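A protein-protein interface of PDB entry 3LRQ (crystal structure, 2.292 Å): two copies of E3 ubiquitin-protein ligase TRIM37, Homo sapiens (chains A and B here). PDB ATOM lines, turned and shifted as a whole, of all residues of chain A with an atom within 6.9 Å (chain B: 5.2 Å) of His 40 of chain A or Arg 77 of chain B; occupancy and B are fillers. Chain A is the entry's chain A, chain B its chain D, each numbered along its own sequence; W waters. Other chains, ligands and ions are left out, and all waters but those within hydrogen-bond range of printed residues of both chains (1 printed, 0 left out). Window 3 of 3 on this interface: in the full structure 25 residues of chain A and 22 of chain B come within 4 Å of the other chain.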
ATOM      1  N   LEU A  37      -5.348  -5.156  30.006  1.00  0.00           N
ATOM      2  CA  LEU A  37      -6.058  -5.609  28.852  1.00  0.00           C
ATOM      3  C   LEU A  37      -7.026  -4.519  28.391  1.00  0.00           C
ATOM      4  O   LEU A  37      -7.722  -3.918  29.202  1.00  0.00           O
ATOM      5  CB  LEU A  37      -6.783  -6.897  29.226  1.00  0.00           C
ATOM      6  CG  LEU A  37      -7.652  -7.588  28.193  1.00  0.00           C
ATOM      7  CD1 LEU A  37      -7.308  -9.085  28.085  1.00  0.00           C
ATOM      8  CD2 LEU A  37      -9.106  -7.354  28.574  1.00  0.00           C
ATOM      9  N   CYS A  38      -7.027  -4.234  27.091  1.00  0.00           N
ATOM     10  CA  CYS A  38      -7.998  -3.319  26.512  1.00  0.00           C
ATOM     11  C   CYS A  38      -9.371  -3.969  26.471  1.00  0.00           C
ATOM     12  O   CYS A  38      -9.544  -5.025  25.859  1.00  0.00           O
ATOM     13  CB  CYS A  38      -7.616  -2.951  25.079  1.00  0.00           C
ATOM     14  SG  CYS A  38      -8.962  -2.026  24.277  1.00  0.00           S
ATOM     15  N   PRO A  39     -10.363  -3.319  27.088  1.00  0.00           N
ATOM     16  CA  PRO A  39     -11.715  -3.864  27.268  1.00  0.00           C
ATOM     17  C   PRO A  39     -12.428  -4.055  25.941  1.00  0.00           C
ATOM     18  O   PRO A  39     -13.342  -4.865  25.848  1.00  0.00           O
ATOM     19  CB  PRO A  39     -12.446  -2.767  28.060  1.00  0.00           C
ATOM     20  CG  PRO A  39     -11.396  -1.818  28.507  1.00  0.00           C
ATOM     21  CD  PRO A  39     -10.257  -1.931  27.554  1.00  0.00           C
ATOM     22  N   HIS A  40     -12.017  -3.316  24.922  1.00  0.00           N
ATOM     23  CA  HIS A  40     -12.750  -3.321  23.659  1.00  0.00           C
ATOM     24  C   HIS A  40     -12.250  -4.352  22.677  1.00  0.00           C
ATOM     25  O   HIS A  40     -13.019  -4.821  21.838  1.00  0.00           O
ATOM     26  CB  HIS A  40     -12.702  -1.944  22.998  1.00  0.00           C
ATOM     27  CG  HIS A  40     -13.056  -0.827  23.924  1.00  0.00           C
ATOM     28  ND1 HIS A  40     -14.296  -0.725  24.528  1.00  0.00           N
ATOM     29  CD2 HIS A  40     -12.327   0.220  24.377  1.00  0.00           C
ATOM     30  CE1 HIS A  40     -14.318   0.349  25.296  1.00  0.00           C
ATOM     31  NE2 HIS A  40     -13.137   0.941  25.222  1.00  0.00           N
ATOM     32  N   CYS A  41     -10.963  -4.679  22.741  1.00  0.00           N
ATOM     33  CA  CYS A  41     -10.404  -5.607  21.768  1.00  0.00           C
ATOM     34  C   CYS A  41      -9.629  -6.764  22.414  1.00  0.00           C
ATOM     35  O   CYS A  41      -9.234  -7.712  21.727  1.00  0.00           O
ATOM     36  CB  CYS A  41      -9.528  -4.856  20.747  1.00  0.00           C
ATOM     37  SG  CYS A  41      -7.860  -4.397  21.343  1.00  0.00           S
ATOM     38  N   SER A  42      -9.378  -6.639  23.719  1.00  0.00           N
ATOM     39  CA  SER A  42      -8.681  -7.635  24.560  1.00  0.00           C
ATOM     40  C   SER A  42      -7.165  -7.757  24.337  1.00  0.00           C
ATOM     41  O   SER A  42      -6.518  -8.669  24.874  1.00  0.00           O
ATOM     42  CB  SER A  42      -9.345  -9.028  24.508  1.00  0.00           C
ATOM     43  OG  SER A  42      -9.068  -9.714  23.292  1.00  0.00           O
ATOM     44  N   LYS A  43      -6.579  -6.854  23.556  1.00  0.00           N
ATOM     45  CA  LYS A  43      -5.120  -6.819  23.476  1.00  0.00           C
ATOM     46  C   LYS A  43      -4.529  -6.513  24.834  1.00  0.00           C
ATOM     47  O   LYS A  43      -5.070  -5.703  25.590  1.00  0.00           O
ATOM     48  CB  LYS A  43      -4.636  -5.805  22.442  1.00  0.00           C
ATOM     49  CG  LYS A  43      -4.729  -6.315  21.021  1.00  0.00           C
ATOM     50  CD  LYS A  43      -3.893  -7.575  20.806  1.00  0.00           C
ATOM     51  CE  LYS A  43      -3.963  -7.964  19.311  1.00  0.00           C
ATOM     52  NZ  LYS A  43      -2.956  -8.990  18.904  1.00  0.00           N
ATOM     53  N   CYS A  61      -6.608   2.916  22.231  1.00  0.00           N
ATOM     54  CA  CYS A  61      -5.942   1.639  22.260  1.00  0.00           C
ATOM     55  C   CYS A  61      -4.934   1.610  21.111  1.00  0.00           C
ATOM     56  O   CYS A  61      -5.274   1.981  19.996  1.00  0.00           O
ATOM     57  CB  CYS A  61      -6.936   0.496  22.092  1.00  0.00           C
ATOM     58  SG  CYS A  61      -6.081  -1.094  22.034  1.00  0.00           S
ATOM     59  N   HIS A  63      -3.816  -0.819  19.551  1.00  0.00           N
ATOM     60  CA  HIS A  63      -4.204  -1.787  18.535  1.00  0.00           C
ATOM     61  C   HIS A  63      -5.533  -1.447  17.889  1.00  0.00           C
ATOM     62  O   HIS A  63      -5.629  -1.384  16.674  1.00  0.00           O
ATOM     63  CB  HIS A  63      -4.279  -3.197  19.115  1.00  0.00           C
ATOM     64  CG  HIS A  63      -4.926  -4.201  18.205  1.00  0.00           C
ATOM     65  ND1 HIS A  63      -6.146  -4.778  18.485  1.00  0.00           N
ATOM     66  CD2 HIS A  63      -4.509  -4.752  17.036  1.00  0.00           C
ATOM     67  CE1 HIS A  63      -6.455  -5.639  17.528  1.00  0.00           C
ATOM     68  NE2 HIS A  63      -5.481  -5.641  16.636  1.00  0.00           N
ATOM     69  N   CYS A  64      -6.573  -1.262  18.684  1.00  0.00           N
ATOM     70  CA  CYS A  64      -7.891  -1.187  18.073  1.00  0.00           C
ATOM     71  C   CYS A  64      -8.336   0.246  17.875  1.00  0.00           C
ATOM     72  O   CYS A  64      -9.340   0.489  17.225  1.00  0.00           O
ATOM     73  CB  CYS A  64      -8.927  -1.966  18.888  1.00  0.00           C
ATOM     74  SG  CYS A  64      -9.544  -1.094  20.334  1.00  0.00           S
ATOM     75  N   ALA A  66      -9.805   2.343  19.690  1.00  0.00           N
ATOM     76  CA  ALA A  66     -10.940   2.814  20.487  1.00  0.00           C
ATOM     77  C   ALA A  66     -10.501   3.819  21.557  1.00  0.00           C
ATOM     78  O   ALA A  66      -9.438   3.657  22.169  1.00  0.00           O
ATOM     79  CB  ALA A  66     -11.666   1.625  21.132  1.00  0.00           C
ATOM     80  N   PRO A  67     -11.305   4.880  21.774  1.00  0.00           N
ATOM     81  CA  PRO A  67     -11.028   5.765  22.906  1.00  0.00           C
ATOM     82  C   PRO A  67     -10.828   4.921  24.134  1.00  0.00           C
ATOM     83  O   PRO A  67     -11.454   3.865  24.259  1.00  0.00           O
ATOM     84  CB  PRO A  67     -12.317   6.579  23.032  1.00  0.00           C
ATOM     85  CG  PRO A  67     -12.808   6.668  21.632  1.00  0.00           C
ATOM     86  CD  PRO A  67     -12.444   5.357  20.971  1.00  0.00           C
ATOM     87  N   LEU A  68      -9.958   5.369  25.026  1.00  0.00           N
ATOM     88  CA  LEU A  68      -9.534   4.530  26.130  1.00  0.00           C
ATOM     89  C   LEU A  68      -8.835   5.399  27.153  1.00  0.00           C
ATOM     90  O   LEU A  68      -7.929   6.150  26.810  1.00  0.00           O
ATOM     91  CB  LEU A  68      -8.576   3.441  25.626  1.00  0.00           C
ATOM     92  CG  LEU A  68      -8.216   2.340  26.613  1.00  0.00           C
ATOM     93  CD1 LEU A  68      -9.438   1.446  26.862  1.00  0.00           C
ATOM     94  CD2 LEU A  68      -7.024   1.505  26.123  1.00  0.00           C
ATOM     95  N   GLN A  69      -9.283   5.315  28.401  1.00  0.00           N
ATOM     96  CA  GLN A  69      -8.605   5.986  29.497  1.00  0.00           C
ATOM     97  C   GLN A  69      -7.966   4.926  30.370  1.00  0.00           C
ATOM     98  O   GLN A  69      -8.421   3.772  30.393  1.00  0.00           O
ATOM     99  CB  GLN A  69      -9.585   6.821  30.324  1.00  0.00           C
ATOM    100  CG  GLN A  69      -9.917   8.176  29.719  1.00  0.00           C
ATOM    101  CD  GLN A  69     -10.790   9.013  30.644  1.00  0.00           C
ATOM    102  OE1 GLN A  69     -11.638   8.481  31.367  1.00  0.00           O
ATOM    103  NE2 GLN A  69     -10.578  10.327  30.633  1.00  0.00           N
ATOM    104  N   GLU A  72     -10.170   2.553  32.366  1.00  0.00           N
ATOM    105  CA  GLU A  72     -11.006   1.541  31.726  1.00  0.00           C
ATOM    106  C   GLU A  72     -10.204   0.257  31.469  1.00  0.00           C
ATOM    107  O   GLU A  72     -10.771  -0.774  31.126  1.00  0.00           O
ATOM    108  CB  GLU A  72     -11.593   2.041  30.401  1.00  0.00           C
ATOM    109  CG  GLU A  72     -12.284   3.383  30.446  1.00  0.00           C
ATOM    110  CD  GLU A  72     -12.391   4.006  29.060  1.00  0.00           C
ATOM    111  OE1 GLU A  72     -12.715   3.274  28.086  1.00  0.00           O
ATOM    112  OE2 GLU A  72     -12.136   5.227  28.945  1.00  0.00           O
ATOM    113  N   ASN B  75     -14.673  -9.668  25.501  1.00  0.00           N
ATOM    114  CA  ASN B  75     -14.473 -10.742  24.530  1.00  0.00           C
ATOM    115  C   ASN B  75     -12.984 -11.065  24.411  1.00  0.00           C
ATOM    116  O   ASN B  75     -12.210 -10.245  23.922  1.00  0.00           O
ATOM    117  CB  ASN B  75     -15.006 -10.278  23.177  1.00  0.00           C
ATOM    118  CG  ASN B  75     -14.975 -11.358  22.126  1.00  0.00           C
ATOM    119  OD1 ASN B  75     -14.202 -12.322  22.206  1.00  0.00           O
ATOM    120  ND2 ASN B  75     -15.818 -11.196  21.114  1.00  0.00           N
ATOM    121  N   CYS B  76     -12.575 -12.234  24.885  1.00  0.00           N
ATOM    122  CA  CYS B  76     -11.174 -12.620  24.815  1.00  0.00           C
ATOM    123  C   CYS B  76     -10.872 -13.282  23.468  1.00  0.00           C
ATOM    124  O   CYS B  76     -11.040 -14.483  23.294  1.00  0.00           O
ATOM    125  CB  CYS B  76     -10.794 -13.529  25.991  1.00  0.00           C
ATOM    126  SG  CYS B  76     -10.839 -12.655  27.573  1.00  0.00           S
ATOM    127  N   ARG B  77     -10.408 -12.478  22.525  1.00  0.00           N
ATOM    128  CA  ARG B  77     -10.285 -12.919  21.140  1.00  0.00           C
ATOM    129  C   ARG B  77      -9.160 -13.932  20.937  1.00  0.00           C
ATOM    130  O   ARG B  77      -9.204 -14.731  20.015  1.00  0.00           O
ATOM    131  CB  ARG B  77     -10.140 -11.708  20.206  1.00  0.00           C
ATOM    132  CG  ARG B  77     -11.312 -10.736  20.327  1.00  0.00           C
ATOM    133  CD  ARG B  77     -11.273  -9.599  19.312  1.00  0.00           C
ATOM    134  NE  ARG B  77     -12.311  -8.610  19.605  1.00  0.00           N
ATOM    135  CZ  ARG B  77     -13.547  -8.643  19.115  1.00  0.00           C
ATOM    136  NH1 ARG B  77     -13.910  -9.609  18.277  1.00  0.00           N
ATOM    137  NH2 ARG B  77     -14.421  -7.704  19.457  1.00  0.00           N
ATOM    138  N   TRP B  78      -8.172 -13.905  21.823  1.00  0.00           N
ATOM    139  CA  TRP B  78      -7.034 -14.806  21.748  1.00  0.00           C
ATOM    140  C   TRP B  78      -7.296 -16.106  22.513  1.00  0.00           C
ATOM    141  O   TRP B  78      -6.458 -17.003  22.515  1.00  0.00           O
ATOM    142  CB  TRP B  78      -5.790 -14.106  22.313  1.00  0.00           C
ATOM    143  CG  TRP B  78      -6.121 -13.285  23.499  1.00  0.00           C
ATOM    144  CD1 TRP B  78      -6.297 -11.931  23.537  1.00  0.00           C
ATOM    145  CD2 TRP B  78      -6.364 -13.760  24.826  1.00  0.00           C
ATOM    146  NE1 TRP B  78      -6.615 -11.530  24.811  1.00  0.00           N
ATOM    147  CE2 TRP B  78      -6.664 -12.630  25.625  1.00  0.00           C
ATOM    148  CE3 TRP B  78      -6.337 -15.020  25.426  1.00  0.00           C
ATOM    149  CZ2 TRP B  78      -6.955 -12.732  26.999  1.00  0.00           C
ATOM    150  CZ3 TRP B  78      -6.625 -15.121  26.790  1.00  0.00           C
ATOM    151  CH2 TRP B  78      -6.931 -13.980  27.557  1.00  0.00           C
ATOM    152  N   ALA B  79      -8.441 -16.210  23.181  1.00  0.00           N
ATOM    153  CA  ALA B  79      -8.648 -17.358  24.054  1.00  0.00           C
ATOM    154  C   ALA B  79      -8.697 -18.673  23.287  1.00  0.00           C
ATOM    155  O   ALA B  79      -8.172 -19.683  23.756  1.00  0.00           O
ATOM    156  CB  ALA B  79      -9.902 -17.191  24.915  1.00  0.00           C
ATOM    157  N   GLU B  80      -9.338 -18.669  22.123  1.00  0.00           N
ATOM    158  CA  GLU B  80      -9.494 -19.898  21.347  1.00  0.00           C
ATOM    159  C   GLU B  80      -8.131 -20.425  20.935  1.00  0.00           C
ATOM    160  O   GLU B  80      -7.820 -21.602  21.119  1.00  0.00           O
ATOM    161  CB  GLU B  80     -10.356 -19.654  20.109  1.00  0.00           C
ATOM    162  CG  GLU B  80     -10.694 -20.939  19.320  1.00  0.00           C
ATOM    163  CD  GLU B  80     -11.585 -20.671  18.093  1.00  0.00           C
ATOM    164  OE1 GLU B  80     -12.245 -19.609  18.048  1.00  0.00           O
ATOM    165  OE2 GLU B  80     -11.625 -21.523  17.172  1.00  0.00           O
ATOM    166  N   GLU B  81      -7.315 -19.532  20.383  1.00  0.00           N
ATOM    167  CA  GLU B  81      -5.940 -19.866  20.033  1.00  0.00           C
ATOM    168  C   GLU B  81      -5.279 -20.588  21.196  1.00  0.00           C
ATOM    169  O   GLU B  81      -4.804 -21.708  21.035  1.00  0.00           O
ATOM    170  CB  GLU B  81      -5.150 -18.605  19.679  1.00  0.00           C
ATOM    171  CG  GLU B  81      -3.633 -18.805  19.574  1.00  0.00           C
ATOM    172  CD  GLU B  81      -3.208 -19.662  18.390  1.00  0.00           C
ATOM    173  OE1 GLU B  81      -4.082 -20.072  17.590  1.00  0.00           O
ATOM    174  OE2 GLU B  81      -1.992 -19.927  18.255  1.00  0.00           O
HETATM  175  O   HOH W   1     -14.461  -6.735  24.502  1.00  0.00           O
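The side-chain hydroxyl of Ser 42 of chain A sits at hydrogen-bond distance from the backbone NH of Arg 77 of chain B. The backbone carbonyl oxygen (O) of Ser 42 of chain A sits at hydrogen-bond distance from the indole nitrogen (NE1) of Trp 78 of chain B (2.9 Å). The backbone carbonyl oxygen (O) of Asn 75 of chain B lies close to the side-chain hydroxyl (OG) of Ser 42 of chain A, 3.2 Å away.
SG of Cys 38 of chain A sits close to N of His 40 of chain A. The side-chain sulfur of Cys 41 of chain A lies close to a ring nitrogen (ND1) of His 63 of chain A. The side-chain sulfur (SG) of Cys 41 of chain A sits close to the backbone NH (N) of Lys 43 of chain A (3.5 Å).
Among the printed residues, pairs that only touch across the chains: Cys 41 of chain A with Arg 77 of chain B (3.7 Å), Leu 37 of chain A with Trp 78 of chain B (3.8 Å), Ser 42 of chain A with Cys 76 of chain B (3.9 Å) and His 40 of chain A with Arg 77 of chain B (3.99 Å).
Of the printed residues of chain B, Leu 37 of chain A touches Trp 78 (3.8 Å). Of the printed residues of chain B, His 40 of chain A touches Arg 77. Of the printed residues of chain B, Cys 41 of chain A touches Arg 77. Printed residues of chain A within 4 Å of Cys 76 of chain B: Ser 42 (3.9 Å). Printed residues of chain A within 4 Å of Arg 77 of chain B: His 40, Cys 41 and Ser 42. Of the printed residues of chain A, Trp 78 of chain B touches Leu 37 (3.8 Å) and Ser 42 (2.9 Å). The nearest printed residue of chain B that does not touch His 40 of chain A is Asn 75 of chain B (5.9 Å). The nearest printed residue of chain B that does not touch Ser 42 of chain A is Ala 79 of chain B (6.5 Å).
Of the 7 printed residues of chain B, 4 touch a printed residue of chain A. Hydrophobic or aromatic side chains of chain B within 4 Å of the printed part of chain A: Trp 78. Of the 15 printed residues of chain A, 4 touch a printed residue of chain B. Hydrophobic or aromatic side chains of chain A that line the printed part of chain B: Leu 37.
No position is printed for both chains. Of the 7 pairs that touch across the chains among the printed residues, none has its exchanged pair printed and touching as well.
Water W1 bridges the backbone carbonyl oxygen (O) of Pro 39 of chain A (2.6 Å) and the backbone NH (N) of Asn 75 of chain B (3.1 Å).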
